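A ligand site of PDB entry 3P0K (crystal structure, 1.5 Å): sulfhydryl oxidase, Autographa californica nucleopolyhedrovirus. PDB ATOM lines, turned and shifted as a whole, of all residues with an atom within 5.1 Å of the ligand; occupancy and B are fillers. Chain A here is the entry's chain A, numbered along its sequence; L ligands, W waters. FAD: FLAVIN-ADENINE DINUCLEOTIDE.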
ATOM      1  N   ARG A  11      -6.629 -11.998   6.608  1.00  0.00           N
ATOM      2  CA  ARG A  11      -7.843 -11.642   5.885  1.00  0.00           C
ATOM      3  C   ARG A  11      -7.858 -12.369   4.544  1.00  0.00           C
ATOM      4  O   ARG A  11      -8.895 -12.860   4.110  1.00  0.00           O
ATOM      5  CB  ARG A  11      -7.924 -10.133   5.640  1.00  0.00           C
ATOM      6  CG  ARG A  11      -9.297  -9.678   5.175  1.00  0.00           C
ATOM      7  CD  ARG A  11      -9.306  -8.217   4.772  1.00  0.00           C
ATOM      8  NE  ARG A  11      -8.839  -8.006   3.403  1.00  0.00           N
ATOM      9  CZ  ARG A  11      -8.399  -6.842   2.939  1.00  0.00           C
ATOM     10  NH1 ARG A  11      -8.359  -5.776   3.728  1.00  0.00           N
ATOM     11  NH2 ARG A  11      -8.009  -6.740   1.673  1.00  0.00           N
ATOM     12  N   TYR A  12      -6.699 -12.429   3.884  1.00  0.00           N
ATOM     13  CA  TYR A  12      -6.602 -13.110   2.596  1.00  0.00           C
ATOM     14  C   TYR A  12      -7.019 -14.575   2.741  1.00  0.00           C
ATOM     15  O   TYR A  12      -7.788 -15.095   1.925  1.00  0.00           O
ATOM     16  CB  TYR A  12      -5.173 -13.061   2.051  1.00  0.00           C
ATOM     17  CG  TYR A  12      -4.737 -11.733   1.448  1.00  0.00           C
ATOM     18  CD1 TYR A  12      -5.624 -10.659   1.318  1.00  0.00           C
ATOM     19  CD2 TYR A  12      -3.436 -11.576   0.959  1.00  0.00           C
ATOM     20  CE1 TYR A  12      -5.216  -9.455   0.725  1.00  0.00           C
ATOM     21  CE2 TYR A  12      -3.026 -10.394   0.362  1.00  0.00           C
ATOM     22  CZ  TYR A  12      -3.918  -9.335   0.238  1.00  0.00           C
ATOM     23  OH  TYR A  12      -3.497  -8.181  -0.372  1.00  0.00           O
ATOM     24  N   PHE A 107     -16.280  -7.706  -3.734  1.00  0.00           N
ATOM     25  CA  PHE A 107     -15.167  -7.721  -4.676  1.00  0.00           C
ATOM     26  C   PHE A 107     -13.864  -7.940  -3.919  1.00  0.00           C
ATOM     27  O   PHE A 107     -12.920  -8.536  -4.443  1.00  0.00           O
ATOM     28  CB  PHE A 107     -15.097  -6.397  -5.444  1.00  0.00           C
ATOM     29  CG  PHE A 107     -15.965  -6.361  -6.658  1.00  0.00           C
ATOM     30  CD1 PHE A 107     -15.718  -7.211  -7.731  1.00  0.00           C
ATOM     31  CD2 PHE A 107     -17.014  -5.447  -6.762  1.00  0.00           C
ATOM     32  CE1 PHE A 107     -16.501  -7.170  -8.887  1.00  0.00           C
ATOM     33  CE2 PHE A 107     -17.798  -5.395  -7.905  1.00  0.00           C
ATOM     34  CZ  PHE A 107     -17.543  -6.263  -8.969  1.00  0.00           C
ATOM     35  N   THR A 108     -13.793  -7.459  -2.674  1.00  0.00           N
ATOM     36  CA  THR A 108     -12.590  -7.647  -1.878  1.00  0.00           C
ATOM     37  C   THR A 108     -12.313  -9.138  -1.708  1.00  0.00           C
ATOM     38  O   THR A 108     -11.159  -9.561  -1.655  1.00  0.00           O
ATOM     39  CB  THR A 108     -12.742  -7.000  -0.497  1.00  0.00           C
ATOM     40  OG1 THR A 108     -12.913  -5.584  -0.661  1.00  0.00           O
ATOM     41  CG2 THR A 108     -11.500  -7.270   0.358  1.00  0.00           C
ATOM     42  N   ILE A 110     -12.860 -11.594  -3.832  1.00  0.00           N
ATOM     43  CA  ILE A 110     -12.208 -12.130  -5.018  1.00  0.00           C
ATOM     44  C   ILE A 110     -10.777 -11.589  -5.167  1.00  0.00           C
ATOM     45  O   ILE A 110      -9.857 -12.355  -5.476  1.00  0.00           O
ATOM     46  CB  ILE A 110     -12.992 -11.771  -6.312  1.00  0.00           C
ATOM     47  CG1 ILE A 110     -14.451 -12.235  -6.210  1.00  0.00           C
ATOM     48  CG2 ILE A 110     -12.335 -12.446  -7.514  1.00  0.00           C
ATOM     49  CD1 ILE A 110     -15.304 -11.374  -5.318  1.00  0.00           C
ATOM     50  N   TRP A 111     -10.571 -10.295  -4.921  1.00  0.00           N
ATOM     51  CA  TRP A 111      -9.214  -9.741  -5.005  1.00  0.00           C
ATOM     52  C   TRP A 111      -8.309 -10.447  -3.988  1.00  0.00           C
ATOM     53  O   TRP A 111      -7.209 -10.876  -4.324  1.00  0.00           O
ATOM     54  CB  TRP A 111      -9.213  -8.233  -4.736  1.00  0.00           C
ATOM     55  CG  TRP A 111      -9.547  -7.393  -5.936  1.00  0.00           C
ATOM     56  CD1 TRP A 111     -10.564  -6.482  -6.052  1.00  0.00           C
ATOM     57  CD2 TRP A 111      -8.862  -7.388  -7.195  1.00  0.00           C
ATOM     58  NE1 TRP A 111     -10.543  -5.903  -7.293  1.00  0.00           N
ATOM     59  CE2 TRP A 111      -9.509  -6.441  -8.022  1.00  0.00           C
ATOM     60  CE3 TRP A 111      -7.760  -8.087  -7.702  1.00  0.00           C
ATOM     61  CZ2 TRP A 111      -9.104  -6.187  -9.338  1.00  0.00           C
ATOM     62  CZ3 TRP A 111      -7.347  -7.828  -9.014  1.00  0.00           C
ATOM     63  CH2 TRP A 111      -8.020  -6.885  -9.807  1.00  0.00           C
ATOM     64  N   ASP A 112      -8.795 -10.573  -2.756  1.00  0.00           N
ATOM     65  CA  ASP A 112      -8.032 -11.239  -1.699  1.00  0.00           C
ATOM     66  C   ASP A 112      -7.647 -12.645  -2.139  1.00  0.00           C
ATOM     67  O   ASP A 112      -6.534 -13.108  -1.872  1.00  0.00           O
ATOM     68  CB  ASP A 112      -8.874 -11.364  -0.427  1.00  0.00           C
ATOM     69  CG  ASP A 112      -8.921 -10.069   0.381  1.00  0.00           C
ATOM     70  OD1 ASP A 112      -8.372  -9.050  -0.068  1.00  0.00           O
ATOM     71  OD2 ASP A 112      -9.524 -10.090   1.471  1.00  0.00           O
ATOM     72  N   MET A 114      -7.169 -13.756  -5.216  1.00  0.00           N
ATOM     73  CA  MET A 114      -6.124 -13.659  -6.220  1.00  0.00           C
ATOM     74  C   MET A 114      -4.781 -13.309  -5.593  1.00  0.00           C
ATOM     75  O   MET A 114      -3.742 -13.847  -5.981  1.00  0.00           O
ATOM     76  CB  MET A 114      -6.516 -12.620  -7.281  1.00  0.00           C
ATOM     77  CG  MET A 114      -7.712 -13.064  -8.116  1.00  0.00           C
ATOM     78  SD  MET A 114      -8.366 -11.800  -9.212  1.00  0.00           S
ATOM     79  CE  MET A 114      -7.146 -11.746 -10.415  1.00  0.00           C
ATOM     80  N   HIS A 115      -4.791 -12.417  -4.610  1.00  0.00           N
ATOM     81  CA  HIS A 115      -3.550 -12.048  -3.947  1.00  0.00           C
ATOM     82  C   HIS A 115      -3.013 -13.218  -3.123  1.00  0.00           C
ATOM     83  O   HIS A 115      -1.810 -13.423  -3.033  1.00  0.00           O
ATOM     84  CB  HIS A 115      -3.765 -10.811  -3.074  1.00  0.00           C
ATOM     85  CG  HIS A 115      -4.030  -9.566  -3.853  1.00  0.00           C
ATOM     86  ND1 HIS A 115      -3.196  -9.141  -4.866  1.00  0.00           N
ATOM     87  CD2 HIS A 115      -5.047  -8.669  -3.802  1.00  0.00           C
ATOM     88  CE1 HIS A 115      -3.685  -8.027  -5.399  1.00  0.00           C
ATOM     89  NE2 HIS A 115      -4.810  -7.722  -4.765  1.00  0.00           N
ATOM     90  N   PHE A 152     -16.890 -15.117 -11.025  1.00  0.00           N
ATOM     91  CA  PHE A 152     -17.145 -13.976 -10.152  1.00  0.00           C
ATOM     92  C   PHE A 152     -18.198 -14.231  -9.076  1.00  0.00           C
ATOM     93  O   PHE A 152     -18.171 -13.611  -8.018  1.00  0.00           O
ATOM     94  CB  PHE A 152     -17.542 -12.754 -10.997  1.00  0.00           C
ATOM     95  CG  PHE A 152     -16.364 -12.081 -11.654  1.00  0.00           C
ATOM     96  CD1 PHE A 152     -15.767 -10.959 -11.079  1.00  0.00           C
ATOM     97  CD2 PHE A 152     -15.832 -12.587 -12.838  1.00  0.00           C
ATOM     98  CE1 PHE A 152     -14.662 -10.357 -11.666  1.00  0.00           C
ATOM     99  CE2 PHE A 152     -14.719 -11.992 -13.435  1.00  0.00           C
ATOM    100  CZ  PHE A 152     -14.127 -10.873 -12.841  1.00  0.00           C
ATOM    101  N   MET A 158     -19.282  -6.506 -17.142  1.00  0.00           N
ATOM    102  CA  MET A 158     -18.198  -5.612 -17.550  1.00  0.00           C
ATOM    103  C   MET A 158     -16.866  -6.106 -16.989  1.00  0.00           C
ATOM    104  O   MET A 158     -15.849  -6.076 -17.684  1.00  0.00           O
ATOM    105  CB  MET A 158     -18.485  -4.192 -17.066  1.00  0.00           C
ATOM    106  CG  MET A 158     -17.372  -3.199 -17.361  1.00  0.00           C
ATOM    107  SD  MET A 158     -17.853  -1.486 -17.026  1.00  0.00           S
ATOM    108  CE  MET A 158     -17.647  -1.421 -15.259  1.00  0.00           C
ATOM    109  N   CYS A 159     -16.878  -6.562 -15.742  1.00  0.00           N
ATOM    110  CA  CYS A 159     -15.669  -7.062 -15.092  1.00  0.00           C
ATOM    111  C   CYS A 159     -15.170  -8.300 -15.836  1.00  0.00           C
ATOM    112  O   CYS A 159     -13.987  -8.443 -16.112  1.00  0.00           O
ATOM    113  CB  CYS A 159     -15.962  -7.483 -13.648  1.00  0.00           C
ATOM    114  SG  CYS A 159     -16.703  -6.259 -12.522  1.00  0.00           S
ATOM    115  N   HIS A 162     -13.686  -7.411 -19.251  1.00  0.00           N
ATOM    116  CA  HIS A 162     -12.392  -6.756 -19.100  1.00  0.00           C
ATOM    117  C   HIS A 162     -11.328  -7.770 -18.681  1.00  0.00           C
ATOM    118  O   HIS A 162     -10.232  -7.787 -19.256  1.00  0.00           O
ATOM    119  CB  HIS A 162     -12.508  -5.624 -18.069  1.00  0.00           C
ATOM    120  CG  HIS A 162     -11.249  -4.851 -17.862  1.00  0.00           C
ATOM    121  ND1 HIS A 162     -11.034  -4.031 -16.772  1.00  0.00           N
ATOM    122  CD2 HIS A 162     -10.112  -4.782 -18.599  1.00  0.00           C
ATOM    123  CE1 HIS A 162      -9.824  -3.511 -16.843  1.00  0.00           C
ATOM    124  NE2 HIS A 162      -9.243  -3.950 -17.946  1.00  0.00           N
ATOM    125  N   TYR A 163     -11.644  -8.602 -17.698  1.00  0.00           N
ATOM    126  CA  TYR A 163     -10.677  -9.606 -17.243  1.00  0.00           C
ATOM    127  C   TYR A 163     -10.301 -10.527 -18.397  1.00  0.00           C
ATOM    128  O   TYR A 163      -9.138 -10.919 -18.527  1.00  0.00           O
ATOM    129  CB  TYR A 163     -11.267 -10.422 -16.085  1.00  0.00           C
ATOM    130  CG  TYR A 163     -10.257 -11.354 -15.453  1.00  0.00           C
ATOM    131  CD1 TYR A 163      -9.205 -10.857 -14.683  1.00  0.00           C
ATOM    132  CD2 TYR A 163     -10.312 -12.730 -15.670  1.00  0.00           C
ATOM    133  CE1 TYR A 163      -8.230 -11.703 -14.152  1.00  0.00           C
ATOM    134  CE2 TYR A 163      -9.343 -13.580 -15.151  1.00  0.00           C
ATOM    135  CZ  TYR A 163      -8.303 -13.055 -14.390  1.00  0.00           C
ATOM    136  OH  TYR A 163      -7.330 -13.902 -13.912  1.00  0.00           O
ATOM    137  N   SER A 222       0.305  -9.083  -9.068  1.00  0.00           N
ATOM    138  CA  SER A 222      -1.115  -8.995  -8.716  1.00  0.00           C
ATOM    139  C   SER A 222      -1.459  -7.599  -8.180  1.00  0.00           C
ATOM    140  O   SER A 222      -2.536  -7.079  -8.468  1.00  0.00           O
ATOM    141  CB  SER A 222      -1.506 -10.098  -7.725  1.00  0.00           C
ATOM    142  OG  SER A 222      -0.910  -9.915  -6.454  1.00  0.00           O
ATOM    143  N   MET A 223      -0.553  -6.993  -7.401  1.00  0.00           N
ATOM    144  CA  MET A 223      -0.795  -5.640  -6.897  1.00  0.00           C
ATOM    145  C   MET A 223      -0.942  -4.659  -8.065  1.00  0.00           C
ATOM    146  O   MET A 223      -1.851  -3.824  -8.089  1.00  0.00           O
ATOM    147  CB  MET A 223       0.365  -5.183  -5.996  1.00  0.00           C
ATOM    148  CG  MET A 223       0.166  -3.744  -5.482  1.00  0.00           C
ATOM    149  SD  MET A 223       1.698  -2.898  -4.965  1.00  0.00           S
ATOM    150  CE  MET A 223       2.331  -2.393  -6.534  1.00  0.00           C
ATOM    151  N   THR A 224      -0.030  -4.764  -9.022  1.00  0.00           N
ATOM    152  CA  THR A 224      -0.017  -3.896 -10.196  1.00  0.00           C
ATOM    153  C   THR A 224      -1.291  -4.095 -11.027  1.00  0.00           C
ATOM    154  O   THR A 224      -1.913  -3.135 -11.493  1.00  0.00           O
ATOM    155  CB  THR A 224       1.237  -4.189 -11.033  1.00  0.00           C
ATOM    156  OG1 THR A 224       2.401  -3.870 -10.265  1.00  0.00           O
ATOM    157  CG2 THR A 224       1.246  -3.381 -12.316  1.00  0.00           C
ATOM    158  N   PHE A 225      -1.669  -5.355 -11.212  1.00  0.00           N
ATOM    159  CA  PHE A 225      -2.868  -5.684 -11.972  1.00  0.00           C
ATOM    160  C   PHE A 225      -4.109  -5.098 -11.296  1.00  0.00           C
ATOM    161  O   PHE A 225      -4.990  -4.557 -11.955  1.00  0.00           O
ATOM    162  CB  PHE A 225      -2.998  -7.203 -12.069  1.00  0.00           C
ATOM    163  CG  PHE A 225      -4.123  -7.650 -12.947  1.00  0.00           C
ATOM    164  CD1 PHE A 225      -3.959  -7.712 -14.325  1.00  0.00           C
ATOM    165  CD2 PHE A 225      -5.341  -8.028 -12.392  1.00  0.00           C
ATOM    166  CE1 PHE A 225      -5.006  -8.145 -15.144  1.00  0.00           C
ATOM    167  CE2 PHE A 225      -6.395  -8.455 -13.202  1.00  0.00           C
ATOM    168  CZ  PHE A 225      -6.229  -8.514 -14.589  1.00  0.00           C
ATOM    169  N   HIS A 226      -4.174  -5.223  -9.968  1.00  0.00           N
ATOM    170  CA  HIS A 226      -5.290  -4.713  -9.183  1.00  0.00           C
ATOM    171  C   HIS A 226      -5.382  -3.188  -9.365  1.00  0.00           C
ATOM    172  O   HIS A 226      -6.479  -2.634  -9.566  1.00  0.00           O
ATOM    173  CB  HIS A 226      -5.084  -5.128  -7.714  1.00  0.00           C
ATOM    174  CG  HIS A 226      -6.256  -4.879  -6.829  1.00  0.00           C
ATOM    175  ND1 HIS A 226      -6.399  -5.511  -5.604  1.00  0.00           N
ATOM    176  CD2 HIS A 226      -7.289  -4.014  -6.927  1.00  0.00           C
ATOM    177  CE1 HIS A 226      -7.482  -5.050  -5.001  1.00  0.00           C
ATOM    178  NE2 HIS A 226      -8.040  -4.141  -5.777  1.00  0.00           N
ATOM    179  N   ASN A 227      -4.246  -2.502  -9.298  1.00  0.00           N
ATOM    180  CA  ASN A 227      -4.237  -1.044  -9.504  1.00  0.00           C
ATOM    181  C   ASN A 227      -4.744  -0.735 -10.905  1.00  0.00           C
ATOM    182  O   ASN A 227      -5.526   0.193 -11.096  1.00  0.00           O
ATOM    183  CB  ASN A 227      -2.824  -0.457  -9.384  1.00  0.00           C
ATOM    184  CG  ASN A 227      -2.431  -0.107  -7.971  1.00  0.00           C
ATOM    185  OD1 ASN A 227      -3.279   0.145  -7.115  1.00  0.00           O
ATOM    186  ND2 ASN A 227      -1.130  -0.052  -7.725  1.00  0.00           N
ATOM    187  N   ILE A 229      -6.796  -2.398 -12.946  1.00  0.00           N
ATOM    188  CA  ILE A 229      -8.238  -2.555 -13.096  1.00  0.00           C
ATOM    189  C   ILE A 229      -8.947  -1.342 -12.495  1.00  0.00           C
ATOM    190  O   ILE A 229      -9.891  -0.793 -13.076  1.00  0.00           O
ATOM    191  CB  ILE A 229      -8.747  -3.835 -12.388  1.00  0.00           C
ATOM    192  CG1 ILE A 229      -8.199  -5.090 -13.079  1.00  0.00           C
ATOM    193  CG2 ILE A 229     -10.268  -3.843 -12.363  1.00  0.00           C
ATOM    194  CD1 ILE A 229      -8.558  -5.194 -14.549  1.00  0.00           C
ATOM    195  N   ASN A 230      -8.498  -0.895 -11.322  1.00  0.00           N
ATOM    196  CA  ASN A 230      -9.150   0.260 -10.715  1.00  0.00           C
ATOM    197  C   ASN A 230      -8.859   1.569 -11.451  1.00  0.00           C
ATOM    198  O   ASN A 230      -9.675   2.498 -11.418  1.00  0.00           O
ATOM    199  CB  ASN A 230      -8.805   0.356  -9.230  1.00  0.00           C
ATOM    200  CG  ASN A 230      -9.513  -0.708  -8.401  1.00  0.00           C
ATOM    201  OD1 ASN A 230     -10.562  -1.207  -8.798  1.00  0.00           O
ATOM    202  ND2 ASN A 230      -8.937  -1.055  -7.253  1.00  0.00           N
ATOM    203  N   LYS A 233     -11.295   1.540 -14.644  1.00  0.00           N
ATOM    204  CA  LYS A 233     -12.746   1.622 -14.504  1.00  0.00           C
ATOM    205  C   LYS A 233     -13.282   3.035 -14.715  1.00  0.00           C
ATOM    206  O   LYS A 233     -14.437   3.212 -15.084  1.00  0.00           O
ATOM    207  CB  LYS A 233     -13.199   1.043 -13.161  1.00  0.00           C
ATOM    208  CG  LYS A 233     -12.733   1.771 -11.939  1.00  0.00           C
ATOM    209  CD  LYS A 233     -13.049   0.925 -10.703  1.00  0.00           C
ATOM    210  CE  LYS A 233     -12.742   1.671  -9.429  1.00  0.00           C
ATOM    211  NZ  LYS A 233     -12.974   0.830  -8.220  1.00  0.00           N
ATOM    212  N   GLN A 236     -13.886   3.328 -18.298  1.00  0.00           N
ATOM    213  CA  GLN A 236     -15.089   2.568 -18.656  1.00  0.00           C
ATOM    214  C   GLN A 236     -16.349   3.381 -18.355  1.00  0.00           C
ATOM    215  O   GLN A 236     -17.348   3.271 -19.053  1.00  0.00           O
ATOM    216  CB  GLN A 236     -15.167   1.261 -17.865  1.00  0.00           C
ATOM    217  CG  GLN A 236     -14.064   0.255 -18.135  1.00  0.00           C
ATOM    218  CD  GLN A 236     -14.126  -0.913 -17.174  1.00  0.00           C
ATOM    219  OE1 GLN A 236     -14.294  -0.722 -15.974  1.00  0.00           O
ATOM    220  NE2 GLN A 236     -13.966  -2.128 -17.687  1.00  0.00           N
ATOM    221  N   ARG A 237     -16.289   4.187 -17.293  1.00  0.00           N
ATOM    222  CA  ARG A 237     -17.428   4.993 -16.882  1.00  0.00           C
ATOM    223  C   ARG A 237     -17.393   6.400 -17.485  1.00  0.00           C
ATOM    224  O   ARG A 237     -18.289   7.217 -17.222  1.00  0.00           O
ATOM    225  CB  ARG A 237     -17.450   5.082 -15.350  1.00  0.00           C
ATOM    226  CG  ARG A 237     -17.462   3.723 -14.667  1.00  0.00           C
ATOM    227  CD  ARG A 237     -17.291   3.839 -13.155  1.00  0.00           C
ATOM    228  NE  ARG A 237     -17.142   2.524 -12.532  1.00  0.00           N
ATOM    229  CZ  ARG A 237     -16.934   2.323 -11.232  1.00  0.00           C
ATOM    230  NH1 ARG A 237     -16.828   3.360 -10.408  1.00  0.00           N
ATOM    231  NH2 ARG A 237     -16.808   1.088 -10.759  1.00  0.00           N
ATOM    232  N   MET A 248      -2.381   1.601  -4.562  1.00  0.00           N
ATOM    233  CA  MET A 248      -1.482   0.904  -3.662  1.00  0.00           C
ATOM    234  C   MET A 248      -0.053   1.024  -4.193  1.00  0.00           C
ATOM    235  O   MET A 248       0.164   0.959  -5.396  1.00  0.00           O
ATOM    236  CB  MET A 248      -1.875  -0.580  -3.577  1.00  0.00           C
ATOM    237  CG  MET A 248      -0.968  -1.449  -2.708  1.00  0.00           C
ATOM    238  SD  MET A 248      -1.105  -1.091  -0.945  1.00  0.00           S
ATOM    239  CE  MET A 248      -2.692  -1.851  -0.610  1.00  0.00           C
ATOM    240  N   TYR A 253       2.641  -2.052   0.214  1.00  0.00           N
ATOM    241  CA  TYR A 253       2.172  -3.429   0.117  1.00  0.00           C
ATOM    242  C   TYR A 253       3.149  -4.381   0.798  1.00  0.00           C
ATOM    243  O   TYR A 253       2.735  -5.284   1.524  1.00  0.00           O
ATOM    244  CB  TYR A 253       1.972  -3.811  -1.350  1.00  0.00           C
ATOM    245  CG  TYR A 253       1.055  -4.995  -1.557  1.00  0.00           C
ATOM    246  CD1 TYR A 253      -0.197  -5.052  -0.948  1.00  0.00           C
ATOM    247  CD2 TYR A 253       1.441  -6.055  -2.385  1.00  0.00           C
ATOM    248  CE1 TYR A 253      -1.044  -6.134  -1.144  1.00  0.00           C
ATOM    249  CE2 TYR A 253       0.588  -7.140  -2.594  1.00  0.00           C
ATOM    250  CZ  TYR A 253      -0.645  -7.174  -1.975  1.00  0.00           C
ATOM    251  OH  TYR A 253      -1.489  -8.242  -2.168  1.00  0.00           O
HETATM  252  PA  FAD L   1     -11.195  -2.674  -3.984  1.00  0.00           P
HETATM  253  O1A FAD L   1     -10.241  -2.681  -5.122  1.00  0.00           O
HETATM  254  O2A FAD L   1     -12.362  -3.615  -4.048  1.00  0.00           O
HETATM  255  O5B FAD L   1     -10.484  -2.986  -2.618  1.00  0.00           O
HETATM  256  C5B FAD L   1     -10.389  -4.300  -2.074  1.00  0.00           C
HETATM  257  C4B FAD L   1      -9.252  -4.295  -1.079  1.00  0.00           C
HETATM  258  O4B FAD L   1      -8.007  -4.324  -1.781  1.00  0.00           O
HETATM  259  C3B FAD L   1      -9.149  -3.120  -0.068  1.00  0.00           C
HETATM  260  O3B FAD L   1      -8.812  -3.676   1.210  1.00  0.00           O
HETATM  261  C2B FAD L   1      -8.070  -2.275  -0.626  1.00  0.00           C
HETATM  262  O2B FAD L   1      -7.277  -1.540   0.262  1.00  0.00           O
HETATM  263  C1B FAD L   1      -7.130  -3.297  -1.310  1.00  0.00           C
HETATM  264  N9A FAD L   1      -6.380  -2.805  -2.431  1.00  0.00           N
HETATM  265  C8A FAD L   1      -6.646  -1.725  -3.318  1.00  0.00           C
HETATM  266  N7A FAD L   1      -5.818  -1.646  -4.317  1.00  0.00           N
HETATM  267  C5A FAD L   1      -4.934  -2.711  -4.133  1.00  0.00           C
HETATM  268  C6A FAD L   1      -3.873  -3.219  -4.912  1.00  0.00           C
HETATM  269  N6A FAD L   1      -3.459  -2.643  -6.044  1.00  0.00           N
HETATM  270  N1A FAD L   1      -3.230  -4.367  -4.456  1.00  0.00           N
HETATM  271  C2A FAD L   1      -3.644  -5.002  -3.326  1.00  0.00           C
HETATM  272  N3A FAD L   1      -4.707  -4.578  -2.511  1.00  0.00           N
HETATM  273  C4A FAD L   1      -5.255  -3.370  -3.042  1.00  0.00           C
HETATM  274  N1  FAD L   1     -14.741  -2.930 -11.635  1.00  0.00           N
HETATM  275  C2  FAD L   1     -15.045  -2.166 -12.734  1.00  0.00           C
HETATM  276  O2  FAD L   1     -15.755  -1.149 -12.641  1.00  0.00           O
HETATM  277  N3  FAD L   1     -14.602  -2.585 -13.982  1.00  0.00           N
HETATM  278  C4  FAD L   1     -13.912  -3.790 -14.257  1.00  0.00           C
HETATM  279  O4  FAD L   1     -13.558  -4.065 -15.449  1.00  0.00           O
HETATM  280  C4X FAD L   1     -13.650  -4.558 -13.139  1.00  0.00           C
HETATM  281  N5  FAD L   1     -12.932  -5.781 -13.366  1.00  0.00           N
HETATM  282  C5X FAD L   1     -12.623  -6.542 -12.222  1.00  0.00           C
HETATM  283  C6  FAD L   1     -11.822  -7.703 -12.349  1.00  0.00           C
HETATM  284  C7  FAD L   1     -11.475  -8.535 -11.250  1.00  0.00           C
HETATM  285  C7M FAD L   1     -10.591  -9.760 -11.481  1.00  0.00           C
HETATM  286  C8  FAD L   1     -11.954  -8.174  -9.951  1.00  0.00           C
HETATM  287  C8M FAD L   1     -11.642  -9.005  -8.713  1.00  0.00           C
HETATM  288  C9  FAD L   1     -12.697  -7.013  -9.753  1.00  0.00           C
HETATM  289  C9A FAD L   1     -13.033  -6.163 -10.846  1.00  0.00           C
HETATM  290  N10 FAD L   1     -13.739  -4.860 -10.736  1.00  0.00           N
HETATM  291  C10 FAD L   1     -14.035  -4.103 -11.846  1.00  0.00           C
HETATM  292  C1' FAD L   1     -14.048  -4.370  -9.435  1.00  0.00           C
HETATM  293  C2' FAD L   1     -13.122  -3.313  -8.889  1.00  0.00           C
HETATM  294  O2' FAD L   1     -11.771  -3.799  -9.118  1.00  0.00           O
HETATM  295  C3' FAD L   1     -13.262  -3.001  -7.433  1.00  0.00           C
HETATM  296  O3' FAD L   1     -13.125  -4.151  -6.610  1.00  0.00           O
HETATM  297  C4' FAD L   1     -14.584  -2.358  -7.004  1.00  0.00           C
HETATM  298  O4' FAD L   1     -14.844  -1.273  -7.941  1.00  0.00           O
HETATM  299  C5' FAD L   1     -14.619  -1.839  -5.624  1.00  0.00           C
HETATM  300  O5' FAD L   1     -13.583  -0.874  -5.436  1.00  0.00           O
HETATM  301  P   FAD L   1     -13.103  -0.423  -4.020  1.00  0.00           P
HETATM  302  O1P FAD L   1     -12.933   1.016  -4.106  1.00  0.00           O
HETATM  303  O2P FAD L   1     -14.000  -1.005  -2.982  1.00  0.00           O
HETATM  304  O3P FAD L   1     -11.702  -1.189  -3.842  1.00  0.00           O
HETATM  305  O   HOH W   1      -6.211  -4.238   1.803  1.00  0.00           O
HETATM  306  O   HOH W   2     -16.210   1.755  -4.486  1.00  0.00           O
HETATM  307  O   HOH W   3     -16.976  -1.974  -9.814  1.00  0.00           O
HETATM  308  O   HOH W   4     -11.468  -1.724 -15.124  1.00  0.00           O
HETATM  309  O   HOH W   5      -6.389   0.046  -6.462  1.00  0.00           O
HETATM  310  O   HOH W   6      -7.585  -7.149  -1.887  1.00  0.00           O
HETATM  311  O   HOH W   7      -9.130   0.730  -3.008  1.00  0.00           O
HETATM  312  O   HOH W   8     -14.506  -4.288  -2.333  1.00  0.00           O
HETATM  313  O   HOH W   9     -11.700  -3.897   2.077  1.00  0.00           O
HETATM  314  O   HOH W  10     -11.161   1.910  -6.444  1.00  0.00           O
HETATM  315  O   HOH W  11     -17.610  -0.303  -7.801  1.00  0.00           O
HETATM  316  O   HOH W  12      -5.292  -6.154  -0.406  1.00  0.00           O
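A ring nitrogen (NE2) of His 226 lies within hydrogen-bond range of an oxygen (O1A) of the ligand (2.7 Å).
OE1 of Gln 236 is in hydrogen-bond range of N3 of the ligand (2.7 Å).
The side-chain amino group (NZ) of Lys 233 is in hydrogen-bond range of an oxygen (O4') of the ligand, 2.8 Å away.
A ring nitrogen (ND1) of His 162 is in hydrogen-bond range of an oxygen (O4) of the ligand.
O of Met 223 lies within hydrogen-bond range of N6A of the ligand (2.9 Å).
OD1 of Asn 230 is in hydrogen-bond range of O2' of the ligand.
The side-chain amide oxygen (OD1) of Asn 227 lies within hydrogen-bond range of a nitrogen (N6A) of the ligand (3.0 Å).
An oxygen (O2') of the ligand lies within hydrogen-bond range of the indole nitrogen (NE1) of Trp 111, 3.0 Å away.
The guanidinium group of Arg 237 lies within hydrogen-bond range of an oxygen (O2) of the ligand (3.1 Å).
The guanidinium group (NH2) of Arg 11 sits at hydrogen-bond distance from an oxygen (O3B) of the ligand (3.2 Å).
A ring nitrogen (NE2) of His 226 lies within hydrogen-bond range of the indole nitrogen (NE1) of Trp 111 (3.4 Å).
A ring nitrogen (NE2) of His 115 lies within hydrogen-bond range of a ring nitrogen (ND1) of His 226.
The side-chain amide oxygen of Gln 236 lies close to the side-chain sulfur of Met 158 (3.8 Å).
The side-chain amino group of Lys 233 is in hydrogen-bond range of the side-chain amide oxygen of Asn 230 (3.2 Å).
The backbone carbonyl oxygen of Met 248 is in hydrogen-bond range of the side-chain amide nitrogen of Asn 227 (2.8 Å).
OD1 of Asp 112 is in salt-bridge range of NH2 of Arg 11 (2.9 Å).
ND1 of His 115 sits at hydrogen-bond distance from OH of Tyr 253.
The side-chain hydroxyl of Tyr 253 lies within hydrogen-bond range of the side-chain hydroxyl of Tyr 12 (2.7 Å).
The side-chain sulfur (SG) of Cys 159 lies close to a nitrogen (N10) of the ligand (3.7 Å).
CB of Phe 107 touches O3' of the ligand, at 3.2 Å.
Thr 108 touches the ligand.
Ile 110 touches the ligand (CG2 to C8M, 3.7 Å).
Met 114 touches the ligand.
NE2 of His 115 touches C2A of the ligand, at 3.3 Å.
Phe 152 touches the ligand.
CE of Met 158 touches O2 of the ligand, at 3.2 Å.
CD1 of Tyr 163 touches C7M of the ligand, 3.7 Å away.
Ile 229 touches the ligand.
Met 248 touches the ligand (CB to C6A, 3.6 Å).
Tyr 253 touches the ligand.
Hydrophobic or aromatic side chains that line the ligand: Phe 107, Ile 110, Trp 111, Met 114, His 115, Phe 152, Met 158, His 162, Tyr 163, Met 223, His 226, Ile 229, Met 248 and Tyr 253.
22 residues have an atom within 4 Å of the ligand: Arg 11, Phe 107, Thr 108, Ile 110, Trp 111, Met 114, His 115, Phe 152, Met 158, Cys 159, His 162, Tyr 163, Met 223, His 226, Asn 227, Ile 229, Asn 230, Lys 233, Gln 236, Arg 237, Met 248 and Tyr 253.
The nearest printed residue that does not touch the ligand is Tyr 12 (4.3 Å).
Water W12 lies within hydrogen-bond range of N3A of the ligand, OH of Tyr 12 and NH2 of Arg 11.
Water W1 lies within hydrogen-bond range of an oxygen (O3B) of the ligand (2.7 Å) and the guanidinium group (NH2) of Arg 11 (3.1 Å).
Water W5 lies within hydrogen-bond range of N7A of the ligand (2.8 Å), ND2 of Asn 230 (2.9 Å) and OD1 of Asn 227 (3.2 Å).
Water W3 bridges O4' of the ligand and NH2 of Arg 237.
Water W11 bridges O4' of the ligand (2.9 Å) and NH2 of Arg 237 (3.4 Å).
Water W10 bridges the side-chain amino group of Lys 233 (2.8 Å) and an oxygen (O1P) of the ligand (3.1 Å).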
